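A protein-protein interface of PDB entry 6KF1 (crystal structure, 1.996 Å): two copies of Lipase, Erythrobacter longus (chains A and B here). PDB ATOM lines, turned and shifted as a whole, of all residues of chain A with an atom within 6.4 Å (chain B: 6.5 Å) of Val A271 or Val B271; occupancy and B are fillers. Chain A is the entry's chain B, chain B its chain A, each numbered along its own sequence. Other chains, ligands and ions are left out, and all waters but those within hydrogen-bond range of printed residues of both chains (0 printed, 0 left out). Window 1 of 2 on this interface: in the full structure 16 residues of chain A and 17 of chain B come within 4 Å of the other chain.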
ATOM      1  N   PRO A 242      23.759 -29.987   9.805  1.00  0.00           N
ATOM      2  CA  PRO A 242      22.597 -29.746   8.972  1.00  0.00           C
ATOM      3  C   PRO A 242      21.737 -28.666   9.636  1.00  0.00           C
ATOM      4  O   PRO A 242      21.554 -28.737  10.887  1.00  0.00           O
ATOM      5  CB  PRO A 242      21.863 -31.098   9.014  1.00  0.00           C
ATOM      6  CG  PRO A 242      23.050 -32.098   9.154  1.00  0.00           C
ATOM      7  CD  PRO A 242      23.895 -31.406  10.199  1.00  0.00           C
ATOM      8  N   THR A 243      21.227 -27.727   8.846  1.00  0.00           N
ATOM      9  CA  THR A 243      20.593 -26.494   9.376  1.00  0.00           C
ATOM     10  C   THR A 243      19.260 -26.246   8.697  1.00  0.00           C
ATOM     11  O   THR A 243      19.141 -26.436   7.439  1.00  0.00           O
ATOM     12  CB  THR A 243      21.528 -25.295   9.194  1.00  0.00           C
ATOM     13  OG1 THR A 243      22.705 -25.533   9.933  1.00  0.00           O
ATOM     14  CG2 THR A 243      20.912 -23.985   9.624  1.00  0.00           C
ATOM     15  N   ILE A 244      18.301 -25.754   9.478  1.00  0.00           N
ATOM     16  CA  ILE A 244      17.057 -25.166   8.957  1.00  0.00           C
ATOM     17  C   ILE A 244      17.041 -23.734   9.463  1.00  0.00           C
ATOM     18  O   ILE A 244      17.023 -23.548  10.699  1.00  0.00           O
ATOM     19  CB  ILE A 244      15.798 -25.909   9.375  1.00  0.00           C
ATOM     20  CG1 ILE A 244      15.753 -27.336   8.800  1.00  0.00           C
ATOM     21  CG2 ILE A 244      14.557 -25.161   8.926  1.00  0.00           C
ATOM     22  CD1 ILE A 244      14.888 -28.212   9.613  1.00  0.00           C
ATOM     23  N   VAL A 245      17.049 -22.765   8.555  1.00  0.00           N
ATOM     24  CA  VAL A 245      16.975 -21.323   8.937  1.00  0.00           C
ATOM     25  C   VAL A 245      15.595 -20.887   8.556  1.00  0.00           C
ATOM     26  O   VAL A 245      15.201 -21.014   7.356  1.00  0.00           O
ATOM     27  CB  VAL A 245      18.024 -20.438   8.250  1.00  0.00           C
ATOM     28  CG1 VAL A 245      17.805 -18.966   8.546  1.00  0.00           C
ATOM     29  CG2 VAL A 245      19.431 -20.839   8.620  1.00  0.00           C
ATOM     30  N   TYR A 260      23.076 -15.604   7.198  1.00  0.00           N
ATOM     31  CA  TYR A 260      23.563 -16.867   7.785  1.00  0.00           C
ATOM     32  C   TYR A 260      23.330 -18.016   6.783  1.00  0.00           C
ATOM     33  O   TYR A 260      24.274 -18.792   6.570  1.00  0.00           O
ATOM     34  CB  TYR A 260      22.926 -17.162   9.152  1.00  0.00           C
ATOM     35  CG  TYR A 260      23.495 -18.391   9.807  1.00  0.00           C
ATOM     36  CD1 TYR A 260      24.841 -18.454  10.083  1.00  0.00           C
ATOM     37  CD2 TYR A 260      22.726 -19.526  10.070  1.00  0.00           C
ATOM     38  CE1 TYR A 260      25.434 -19.592  10.604  1.00  0.00           C
ATOM     39  CE2 TYR A 260      23.309 -20.661  10.621  1.00  0.00           C
ATOM     40  CZ  TYR A 260      24.655 -20.695  10.923  1.00  0.00           C
ATOM     41  OH  TYR A 260      25.292 -21.802  11.457  1.00  0.00           O
ATOM     42  N   ALA A 261      22.151 -18.130   6.196  1.00  0.00           N
ATOM     43  CA  ALA A 261      21.846 -19.226   5.236  1.00  0.00           C
ATOM     44  C   ALA A 261      22.784 -19.111   4.023  1.00  0.00           C
ATOM     45  O   ALA A 261      23.373 -20.139   3.601  1.00  0.00           O
ATOM     46  CB  ALA A 261      20.417 -19.210   4.841  1.00  0.00           C
ATOM     47  N   LYS A 262      23.045 -17.892   3.552  1.00  0.00           N
ATOM     48  CA  LYS A 262      24.005 -17.663   2.441  1.00  0.00           C
ATOM     49  C   LYS A 262      25.405 -18.124   2.826  1.00  0.00           C
ATOM     50  O   LYS A 262      26.084 -18.723   1.960  1.00  0.00           O
ATOM     51  CB  LYS A 262      24.021 -16.197   1.996  1.00  0.00           C
ATOM     52  CG  LYS A 262      22.750 -15.789   1.306  1.00  0.00           C
ATOM     53  CD  LYS A 262      22.632 -14.303   1.059  1.00  0.00           C
ATOM     54  CE  LYS A 262      23.734 -13.834   0.142  1.00  0.00           C
ATOM     55  NZ  LYS A 262      23.725 -12.356  -0.045  1.00  0.00           N
ATOM     56  N   LEU A 264      26.216 -20.433   4.946  1.00  0.00           N
ATOM     57  CA  LEU A 264      26.214 -21.920   4.994  1.00  0.00           C
ATOM     58  C   LEU A 264      26.338 -22.472   3.559  1.00  0.00           C
ATOM     59  O   LEU A 264      27.179 -23.303   3.381  1.00  0.00           O
ATOM     60  CB  LEU A 264      24.983 -22.463   5.723  1.00  0.00           C
ATOM     61  CG  LEU A 264      24.934 -22.272   7.228  1.00  0.00           C
ATOM     62  CD1 LEU A 264      23.715 -22.938   7.842  1.00  0.00           C
ATOM     63  CD2 LEU A 264      26.176 -22.761   7.914  1.00  0.00           C
ATOM     64  N   VAL A 265      25.588 -21.967   2.592  1.00  0.00           N
ATOM     65  CA  VAL A 265      25.702 -22.368   1.163  1.00  0.00           C
ATOM     66  C   VAL A 265      27.140 -22.066   0.715  1.00  0.00           C
ATOM     67  O   VAL A 265      27.765 -22.950   0.135  1.00  0.00           O
ATOM     68  CB  VAL A 265      24.656 -21.674   0.287  1.00  0.00           C
ATOM     69  CG1 VAL A 265      24.846 -22.046  -1.193  1.00  0.00           C
ATOM     70  CG2 VAL A 265      23.268 -22.025   0.767  1.00  0.00           C
ATOM     71  N   ARG A 269      27.498 -26.227   3.052  1.00  0.00           N
ATOM     72  CA  ARG A 269      26.746 -26.916   4.130  1.00  0.00           C
ATOM     73  C   ARG A 269      25.295 -27.115   3.695  1.00  0.00           C
ATOM     74  O   ARG A 269      24.718 -26.247   3.030  1.00  0.00           O
ATOM     75  CB  ARG A 269      26.845 -26.120   5.449  1.00  0.00           C
ATOM     76  CG  ARG A 269      28.263 -25.726   5.818  1.00  0.00           C
ATOM     77  CD  ARG A 269      29.299 -26.818   5.754  1.00  0.00           C
ATOM     78  NE  ARG A 269      28.964 -27.921   6.641  1.00  0.00           N
ATOM     79  CZ  ARG A 269      29.345 -29.165   6.463  1.00  0.00           C
ATOM     80  NH1 ARG A 269      30.064 -29.505   5.401  1.00  0.00           N
ATOM     81  NH2 ARG A 269      29.020 -30.065   7.365  1.00  0.00           N
ATOM     82  N   ASP A 270      24.685 -28.212   4.099  1.00  0.00           N
ATOM     83  CA  ASP A 270      23.276 -28.452   3.779  1.00  0.00           C
ATOM     84  C   ASP A 270      22.435 -27.490   4.634  1.00  0.00           C
ATOM     85  O   ASP A 270      22.584 -27.489   5.866  1.00  0.00           O
ATOM     86  CB  ASP A 270      22.909 -29.905   4.050  1.00  0.00           C
ATOM     87  CG  ASP A 270      23.659 -30.932   3.191  1.00  0.00           C
ATOM     88  OD1 ASP A 270      24.327 -30.543   2.192  1.00  0.00           O
ATOM     89  OD2 ASP A 270      23.707 -32.068   3.637  1.00  0.00           O
ATOM     90  N   VAL A 271      21.454 -26.852   4.013  1.00  0.00           N
ATOM     91  CA  VAL A 271      20.578 -25.885   4.718  1.00  0.00           C
ATOM     92  C   VAL A 271      19.242 -25.792   4.017  1.00  0.00           C
ATOM     93  O   VAL A 271      19.189 -25.879   2.784  1.00  0.00           O
ATOM     94  CB  VAL A 271      21.281 -24.525   4.851  1.00  0.00           C
ATOM     95  CG1 VAL A 271      21.869 -24.015   3.561  1.00  0.00           C
ATOM     96  CG2 VAL A 271      20.355 -23.510   5.490  1.00  0.00           C
ATOM     97  N   VAL A 272      18.173 -25.806   4.809  1.00  0.00           N
ATOM     98  CA  VAL A 272      16.808 -25.466   4.354  1.00  0.00           C
ATOM     99  C   VAL A 272      16.622 -24.000   4.756  1.00  0.00           C
ATOM    100  O   VAL A 272      16.767 -23.704   5.946  1.00  0.00           O
ATOM    101  CB  VAL A 272      15.746 -26.364   4.993  1.00  0.00           C
ATOM    102  CG1 VAL A 272      14.367 -26.000   4.500  1.00  0.00           C
ATOM    103  CG2 VAL A 272      16.057 -27.856   4.785  1.00  0.00           C
ATOM    104  N   TYR A 273      16.325 -23.135   3.796  1.00  0.00           N
ATOM    105  CA  TYR A 273      15.996 -21.708   4.035  1.00  0.00           C
ATOM    106  C   TYR A 273      14.521 -21.522   3.739  1.00  0.00           C
ATOM    107  O   TYR A 273      14.065 -21.831   2.646  1.00  0.00           O
ATOM    108  CB  TYR A 273      16.864 -20.722   3.240  1.00  0.00           C
ATOM    109  CG  TYR A 273      16.485 -19.278   3.528  1.00  0.00           C
ATOM    110  CD1 TYR A 273      16.836 -18.708   4.731  1.00  0.00           C
ATOM    111  CD2 TYR A 273      15.664 -18.549   2.675  1.00  0.00           C
ATOM    112  CE1 TYR A 273      16.482 -17.396   5.052  1.00  0.00           C
ATOM    113  CE2 TYR A 273      15.291 -17.234   2.969  1.00  0.00           C
ATOM    114  CZ  TYR A 273      15.699 -16.664   4.175  1.00  0.00           C
ATOM    115  OH  TYR A 273      15.333 -15.425   4.578  1.00  0.00           O
ATOM    116  N   LEU A 274      13.758 -21.180   4.788  1.00  0.00           N
ATOM    117  CA  LEU A 274      12.294 -20.926   4.741  1.00  0.00           C
ATOM    118  C   LEU A 274      12.095 -19.471   5.204  1.00  0.00           C
ATOM    119  O   LEU A 274      12.415 -19.133   6.368  1.00  0.00           O
ATOM    120  CB  LEU A 274      11.500 -21.884   5.627  1.00  0.00           C
ATOM    121  CG  LEU A 274      11.693 -23.389   5.366  1.00  0.00           C
ATOM    122  CD1 LEU A 274      10.841 -24.180   6.312  1.00  0.00           C
ATOM    123  CD2 LEU A 274      11.351 -23.761   3.933  1.00  0.00           C
ATOM    124  N   MET A 307      14.981 -33.545   7.533  1.00  0.00           N
ATOM    125  CA  MET A 307      16.445 -33.365   7.722  1.00  0.00           C
ATOM    126  C   MET A 307      16.984 -34.358   8.748  1.00  0.00           C
ATOM    127  O   MET A 307      18.175 -34.651   8.664  1.00  0.00           O
ATOM    128  CB  MET A 307      16.807 -31.923   8.111  1.00  0.00           C
ATOM    129  CG  MET A 307      16.573 -30.938   6.989  1.00  0.00           C
ATOM    130  SD  MET A 307      17.736 -31.103   5.598  1.00  0.00           S
ATOM    131  CE  MET A 307      19.127 -30.123   6.157  1.00  0.00           C
ATOM    132  N   PRO B 242       9.424 -22.593  -5.163  1.00  0.00           N
ATOM    133  CA  PRO B 242      10.119 -23.383  -4.160  1.00  0.00           C
ATOM    134  C   PRO B 242      11.174 -24.224  -4.921  1.00  0.00           C
ATOM    135  O   PRO B 242      10.861 -24.725  -6.003  1.00  0.00           O
ATOM    136  CB  PRO B 242       9.016 -24.225  -3.512  1.00  0.00           C
ATOM    137  CG  PRO B 242       7.732 -23.391  -3.747  1.00  0.00           C
ATOM    138  CD  PRO B 242       7.968 -22.774  -5.106  1.00  0.00           C
ATOM    139  N   THR B 243      12.386 -24.279  -4.384  1.00  0.00           N
ATOM    140  CA  THR B 243      13.585 -24.826  -5.070  1.00  0.00           C
ATOM    141  C   THR B 243      14.276 -25.864  -4.174  1.00  0.00           C
ATOM    142  O   THR B 243      14.499 -25.603  -2.962  1.00  0.00           O
ATOM    143  CB  THR B 243      14.544 -23.700  -5.480  1.00  0.00           C
ATOM    144  OG1 THR B 243      13.767 -22.842  -6.314  1.00  0.00           O
ATOM    145  CG2 THR B 243      15.780 -24.225  -6.223  1.00  0.00           C
ATOM    146  N   ILE B 244      14.770 -26.917  -4.803  1.00  0.00           N
ATOM    147  CA  ILE B 244      15.830 -27.778  -4.226  1.00  0.00           C
ATOM    148  C   ILE B 244      17.022 -27.685  -5.172  1.00  0.00           C
ATOM    149  O   ILE B 244      16.860 -28.076  -6.329  1.00  0.00           O
ATOM    150  CB  ILE B 244      15.357 -29.225  -4.071  1.00  0.00           C
ATOM    151  CG1 ILE B 244      14.159 -29.247  -3.116  1.00  0.00           C
ATOM    152  CG2 ILE B 244      16.538 -30.122  -3.594  1.00  0.00           C
ATOM    153  CD1 ILE B 244      13.301 -30.441  -3.292  1.00  0.00           C
ATOM    154  N   VAL B 245      18.145 -27.177  -4.691  1.00  0.00           N
ATOM    155  CA  VAL B 245      19.431 -27.152  -5.431  1.00  0.00           C
ATOM    156  C   VAL B 245      20.297 -28.253  -4.827  1.00  0.00           C
ATOM    157  O   VAL B 245      20.529 -28.246  -3.610  1.00  0.00           O
ATOM    158  CB  VAL B 245      20.174 -25.808  -5.346  1.00  0.00           C
ATOM    159  CG1 VAL B 245      21.492 -25.912  -6.088  1.00  0.00           C
ATOM    160  CG2 VAL B 245      19.354 -24.648  -5.881  1.00  0.00           C
ATOM    161  N   TYR B 260      23.664 -20.009  -7.145  1.00  0.00           N
ATOM    162  CA  TYR B 260      22.216 -19.926  -7.380  1.00  0.00           C
ATOM    163  C   TYR B 260      21.414 -19.997  -6.059  1.00  0.00           C
ATOM    164  O   TYR B 260      20.467 -19.201  -5.830  1.00  0.00           O
ATOM    165  CB  TYR B 260      21.771 -20.975  -8.391  1.00  0.00           C
ATOM    166  CG  TYR B 260      20.323 -20.816  -8.731  1.00  0.00           C
ATOM    167  CD1 TYR B 260      19.855 -19.655  -9.328  1.00  0.00           C
ATOM    168  CD2 TYR B 260      19.396 -21.785  -8.400  1.00  0.00           C
ATOM    169  CE1 TYR B 260      18.517 -19.488  -9.616  1.00  0.00           C
ATOM    170  CE2 TYR B 260      18.055 -21.655  -8.746  1.00  0.00           C
ATOM    171  CZ  TYR B 260      17.599 -20.480  -9.310  1.00  0.00           C
ATOM    172  OH  TYR B 260      16.274 -20.310  -9.617  1.00  0.00           O
ATOM    173  N   ALA B 261      21.712 -20.950  -5.207  1.00  0.00           N
ATOM    174  CA  ALA B 261      21.019 -21.093  -3.896  1.00  0.00           C
ATOM    175  C   ALA B 261      21.215 -19.782  -3.100  1.00  0.00           C
ATOM    176  O   ALA B 261      20.227 -19.270  -2.515  1.00  0.00           O
ATOM    177  CB  ALA B 261      21.576 -22.283  -3.176  1.00  0.00           C
ATOM    178  N   LYS B 262      22.410 -19.211  -3.133  1.00  0.00           N
ATOM    179  CA  LYS B 262      22.678 -17.947  -2.386  1.00  0.00           C
ATOM    180  C   LYS B 262      21.824 -16.814  -2.954  1.00  0.00           C
ATOM    181  O   LYS B 262      21.278 -16.012  -2.166  1.00  0.00           O
ATOM    182  CB  LYS B 262      24.155 -17.573  -2.384  1.00  0.00           C
ATOM    183  CG  LYS B 262      25.037 -18.444  -1.527  1.00  0.00           C
ATOM    184  CD  LYS B 262      26.510 -18.188  -1.772  1.00  0.00           C
ATOM    185  CE  LYS B 262      26.905 -16.795  -1.326  1.00  0.00           C
ATOM    186  NZ  LYS B 262      28.286 -16.459  -1.729  1.00  0.00           N
ATOM    187  N   LEU B 264      18.871 -17.189  -4.414  1.00  0.00           N
ATOM    188  CA  LEU B 264      17.474 -17.420  -3.956  1.00  0.00           C
ATOM    189  C   LEU B 264      17.303 -16.932  -2.494  1.00  0.00           C
ATOM    190  O   LEU B 264      16.324 -16.206  -2.239  1.00  0.00           O
ATOM    191  CB  LEU B 264      17.114 -18.894  -4.072  1.00  0.00           C
ATOM    192  CG  LEU B 264      16.995 -19.426  -5.477  1.00  0.00           C
ATOM    193  CD1 LEU B 264      16.527 -20.845  -5.494  1.00  0.00           C
ATOM    194  CD2 LEU B 264      16.065 -18.566  -6.283  1.00  0.00           C
ATOM    195  N   VAL B 265      18.246 -17.210  -1.599  1.00  0.00           N
ATOM    196  CA  VAL B 265      18.154 -16.697  -0.194  1.00  0.00           C
ATOM    197  C   VAL B 265      18.159 -15.154  -0.204  1.00  0.00           C
ATOM    198  O   VAL B 265      17.357 -14.549   0.518  1.00  0.00           O
ATOM    199  CB  VAL B 265      19.279 -17.250   0.676  1.00  0.00           C
ATOM    200  CG1 VAL B 265      19.233 -16.661   2.089  1.00  0.00           C
ATOM    201  CG2 VAL B 265      19.248 -18.779   0.723  1.00  0.00           C
ATOM    202  N   ARG B 269      13.622 -16.283  -1.111  1.00  0.00           N
ATOM    203  CA  ARG B 269      12.863 -17.426  -1.694  1.00  0.00           C
ATOM    204  C   ARG B 269      13.142 -18.707  -0.890  1.00  0.00           C
ATOM    205  O   ARG B 269      14.220 -18.873  -0.387  1.00  0.00           O
ATOM    206  CB  ARG B 269      13.308 -17.629  -3.148  1.00  0.00           C
ATOM    207  CG  ARG B 269      13.151 -16.381  -4.004  1.00  0.00           C
ATOM    208  CD  ARG B 269      11.860 -15.637  -3.786  1.00  0.00           C
ATOM    209  NE  ARG B 269      10.738 -16.411  -4.245  1.00  0.00           N
ATOM    210  CZ  ARG B 269       9.502 -16.279  -3.806  1.00  0.00           C
ATOM    211  NH1 ARG B 269       9.208 -15.376  -2.884  1.00  0.00           N
ATOM    212  NH2 ARG B 269       8.557 -16.999  -4.333  1.00  0.00           N
ATOM    213  N   ASP B 270      12.200 -19.621  -0.809  1.00  0.00           N
ATOM    214  CA  ASP B 270      12.407 -20.860  -0.026  1.00  0.00           C
ATOM    215  C   ASP B 270      13.312 -21.824  -0.831  1.00  0.00           C
ATOM    216  O   ASP B 270      13.017 -22.021  -1.999  1.00  0.00           O
ATOM    217  CB  ASP B 270      11.077 -21.509   0.231  1.00  0.00           C
ATOM    218  CG  ASP B 270      10.176 -20.720   1.165  1.00  0.00           C
ATOM    219  OD1 ASP B 270      10.667 -19.810   1.841  1.00  0.00           O
ATOM    220  OD2 ASP B 270       8.986 -21.019   1.138  1.00  0.00           O
ATOM    221  N   VAL B 271      14.367 -22.353  -0.219  1.00  0.00           N
ATOM    222  CA  VAL B 271      15.327 -23.224  -0.942  1.00  0.00           C
ATOM    223  C   VAL B 271      15.938 -24.226   0.027  1.00  0.00           C
ATOM    224  O   VAL B 271      16.284 -23.855   1.122  1.00  0.00           O
ATOM    225  CB  VAL B 271      16.374 -22.375  -1.690  1.00  0.00           C
ATOM    226  CG1 VAL B 271      17.092 -21.391  -0.776  1.00  0.00           C
ATOM    227  CG2 VAL B 271      17.411 -23.220  -2.431  1.00  0.00           C
ATOM    228  N   VAL B 272      15.994 -25.486  -0.416  1.00  0.00           N
ATOM    229  CA  VAL B 272      16.817 -26.578   0.125  1.00  0.00           C
ATOM    230  C   VAL B 272      18.102 -26.666  -0.704  1.00  0.00           C
ATOM    231  O   VAL B 272      18.028 -26.853  -1.940  1.00  0.00           O
ATOM    232  CB  VAL B 272      16.028 -27.893   0.134  1.00  0.00           C
ATOM    233  CG1 VAL B 272      16.850 -28.962   0.854  1.00  0.00           C
ATOM    234  CG2 VAL B 272      14.674 -27.717   0.787  1.00  0.00           C
ATOM    235  N   TYR B 273      19.220 -26.421  -0.053  1.00  0.00           N
ATOM    236  CA  TYR B 273      20.551 -26.606  -0.613  1.00  0.00           C
ATOM    237  C   TYR B 273      21.171 -27.872  -0.033  1.00  0.00           C
ATOM    238  O   TYR B 273      21.422 -27.935   1.166  1.00  0.00           O
ATOM    239  CB  TYR B 273      21.414 -25.371  -0.354  1.00  0.00           C
ATOM    240  CG  TYR B 273      22.768 -25.561  -0.972  1.00  0.00           C
ATOM    241  CD1 TYR B 273      22.902 -25.491  -2.335  1.00  0.00           C
ATOM    242  CD2 TYR B 273      23.873 -25.936  -0.212  1.00  0.00           C
ATOM    243  CE1 TYR B 273      24.134 -25.689  -2.946  1.00  0.00           C
ATOM    244  CE2 TYR B 273      25.111 -26.165  -0.815  1.00  0.00           C
ATOM    245  CZ  TYR B 273      25.234 -26.051  -2.196  1.00  0.00           C
ATOM    246  OH  TYR B 273      26.397 -26.320  -2.873  1.00  0.00           O
ATOM    247  N   LEU B 274      21.417 -28.854  -0.888  1.00  0.00           N
ATOM    248  CA  LEU B 274      22.092 -30.126  -0.495  1.00  0.00           C
ATOM    249  C   LEU B 274      23.381 -30.249  -1.293  1.00  0.00           C
ATOM    250  O   LEU B 274      23.325 -30.358  -2.523  1.00  0.00           O
ATOM    251  CB  LEU B 274      21.170 -31.305  -0.812  1.00  0.00           C
ATOM    252  CG  LEU B 274      19.812 -31.265  -0.098  1.00  0.00           C
ATOM    253  CD1 LEU B 274      18.987 -32.481  -0.458  1.00  0.00           C
ATOM    254  CD2 LEU B 274      19.993 -31.190   1.405  1.00  0.00           C
ATOM    255  N   MET B 307       8.974 -30.681   0.239  1.00  0.00           N
ATOM    256  CA  MET B 307       8.714 -29.326  -0.317  1.00  0.00           C
ATOM    257  C   MET B 307       7.383 -29.351  -1.066  1.00  0.00           C
ATOM    258  O   MET B 307       6.811 -28.270  -1.206  1.00  0.00           O
ATOM    259  CB  MET B 307       9.842 -28.837  -1.223  1.00  0.00           C
ATOM    260  CG  MET B 307      11.120 -28.527  -0.500  1.00  0.00           C
ATOM    261  SD  MET B 307      11.054 -27.095   0.621  1.00  0.00           S
ATOM    262  CE  MET B 307      11.286 -25.778  -0.573  1.00  0.00           C
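Of the 16 printed residues of chain A, 9 touch a printed residue of chain B.
Of the 16 printed residues of chain B, 9 touch a printed residue of chain A.
Among the printed residues, no Asp or Glu carboxylate lies within 4 Å of a Lys or Arg side-chain nitrogen of the other chain.
Lys A262 touches Lys B262 (O to CG, 3.7 Å).
Tyr B273 touches Val A265.
O of Tyr B273 touches CA of Asp A270, 3.2 Å away.
OD1 of Asp A270 touches CA of Leu B274, 3.5 Å away.
O of Val A271 touches CA of Val B272 (3.6 Å).
Val A272 touches Val B271.
Tyr A273 touches Val B265 (CG to CG2, 3.97 Å).
Arg B269 touches Tyr A273 (O to CD2, 3.4 Å).
CA of Asp B270 touches O of Tyr A273, at 3.3 Å.
OD1 of Asp B270 touches CA of Leu A274, at 3.5 Å.
Lys A262 touches Val B265, and with the chains exchanged Val A265 touches Lys B262.
Arg A269 touches Tyr B273, and with the chains exchanged Tyr A273 touches Arg B269.
Val A271 touches Val B272, and with the chains exchanged Val A272 touches Val B271.
Val A271 touches Tyr B273, and with the chains exchanged Tyr A273 touches Val B271.
Positions printed for both chains: 242, 243, 244, 245, 260, 261, 262, 264, 265, 269, 270, 271, 272, 273, 274 and 307.
Of the 18 pairs that touch across the chains among the printed residues, 18 have their exchanged pair printed and touching as well.
The backbone carbonyl oxygen (O) of Val B271 sits at hydrogen-bond distance from the backbone NH (N) of Tyr A273 (2.8 Å).
The backbone NH of Tyr B273 is in hydrogen-bond range of the backbone carbonyl oxygen of Val A271 (2.9 Å).
O of Asp B270 lies within hydrogen-bond range of N of Thr B243 (3.3 Å).
O of Thr B243 lies within hydrogen-bond range of N of Val B272 (3.0 Å).
The backbone NH of Val B245 sits at hydrogen-bond distance from the backbone carbonyl oxygen of Val B272.
N of Val A272 sits at hydrogen-bond distance from O of Thr A243 (2.9 Å).
The backbone NH (N) of Val A245 lies within hydrogen-bond range of the backbone carbonyl oxygen (O) of Val A272, at 2.8 Å.
The backbone carbonyl oxygen (O) of Val A245 lies within hydrogen-bond range of the backbone NH (N) of Leu A274, at 3.0 Å.
Printed residues of chain B within 4 Å of Lys A262: Lys B262 (3.7 Å) and Val B265 (3.7 Å).
Printed residues of chain B within 4 Å of Val A271: Val B271, Val B272 and Tyr B273.
Of the printed residues of chain B, Leu A274 touches Asp B270 (3.5 Å).
Of the printed residues of chain A, Ala B261 touches Val A265.
Of chain A, only Val A271, Val A272 and Tyr A273 come within 4 Å of Val B271.
The nearest residue of chain A that does not touch Val B271 is Leu A274 (5.2 Å).
The nearest printed residue of chain B that does not touch Val A265 is Val B265 (5.2 Å).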
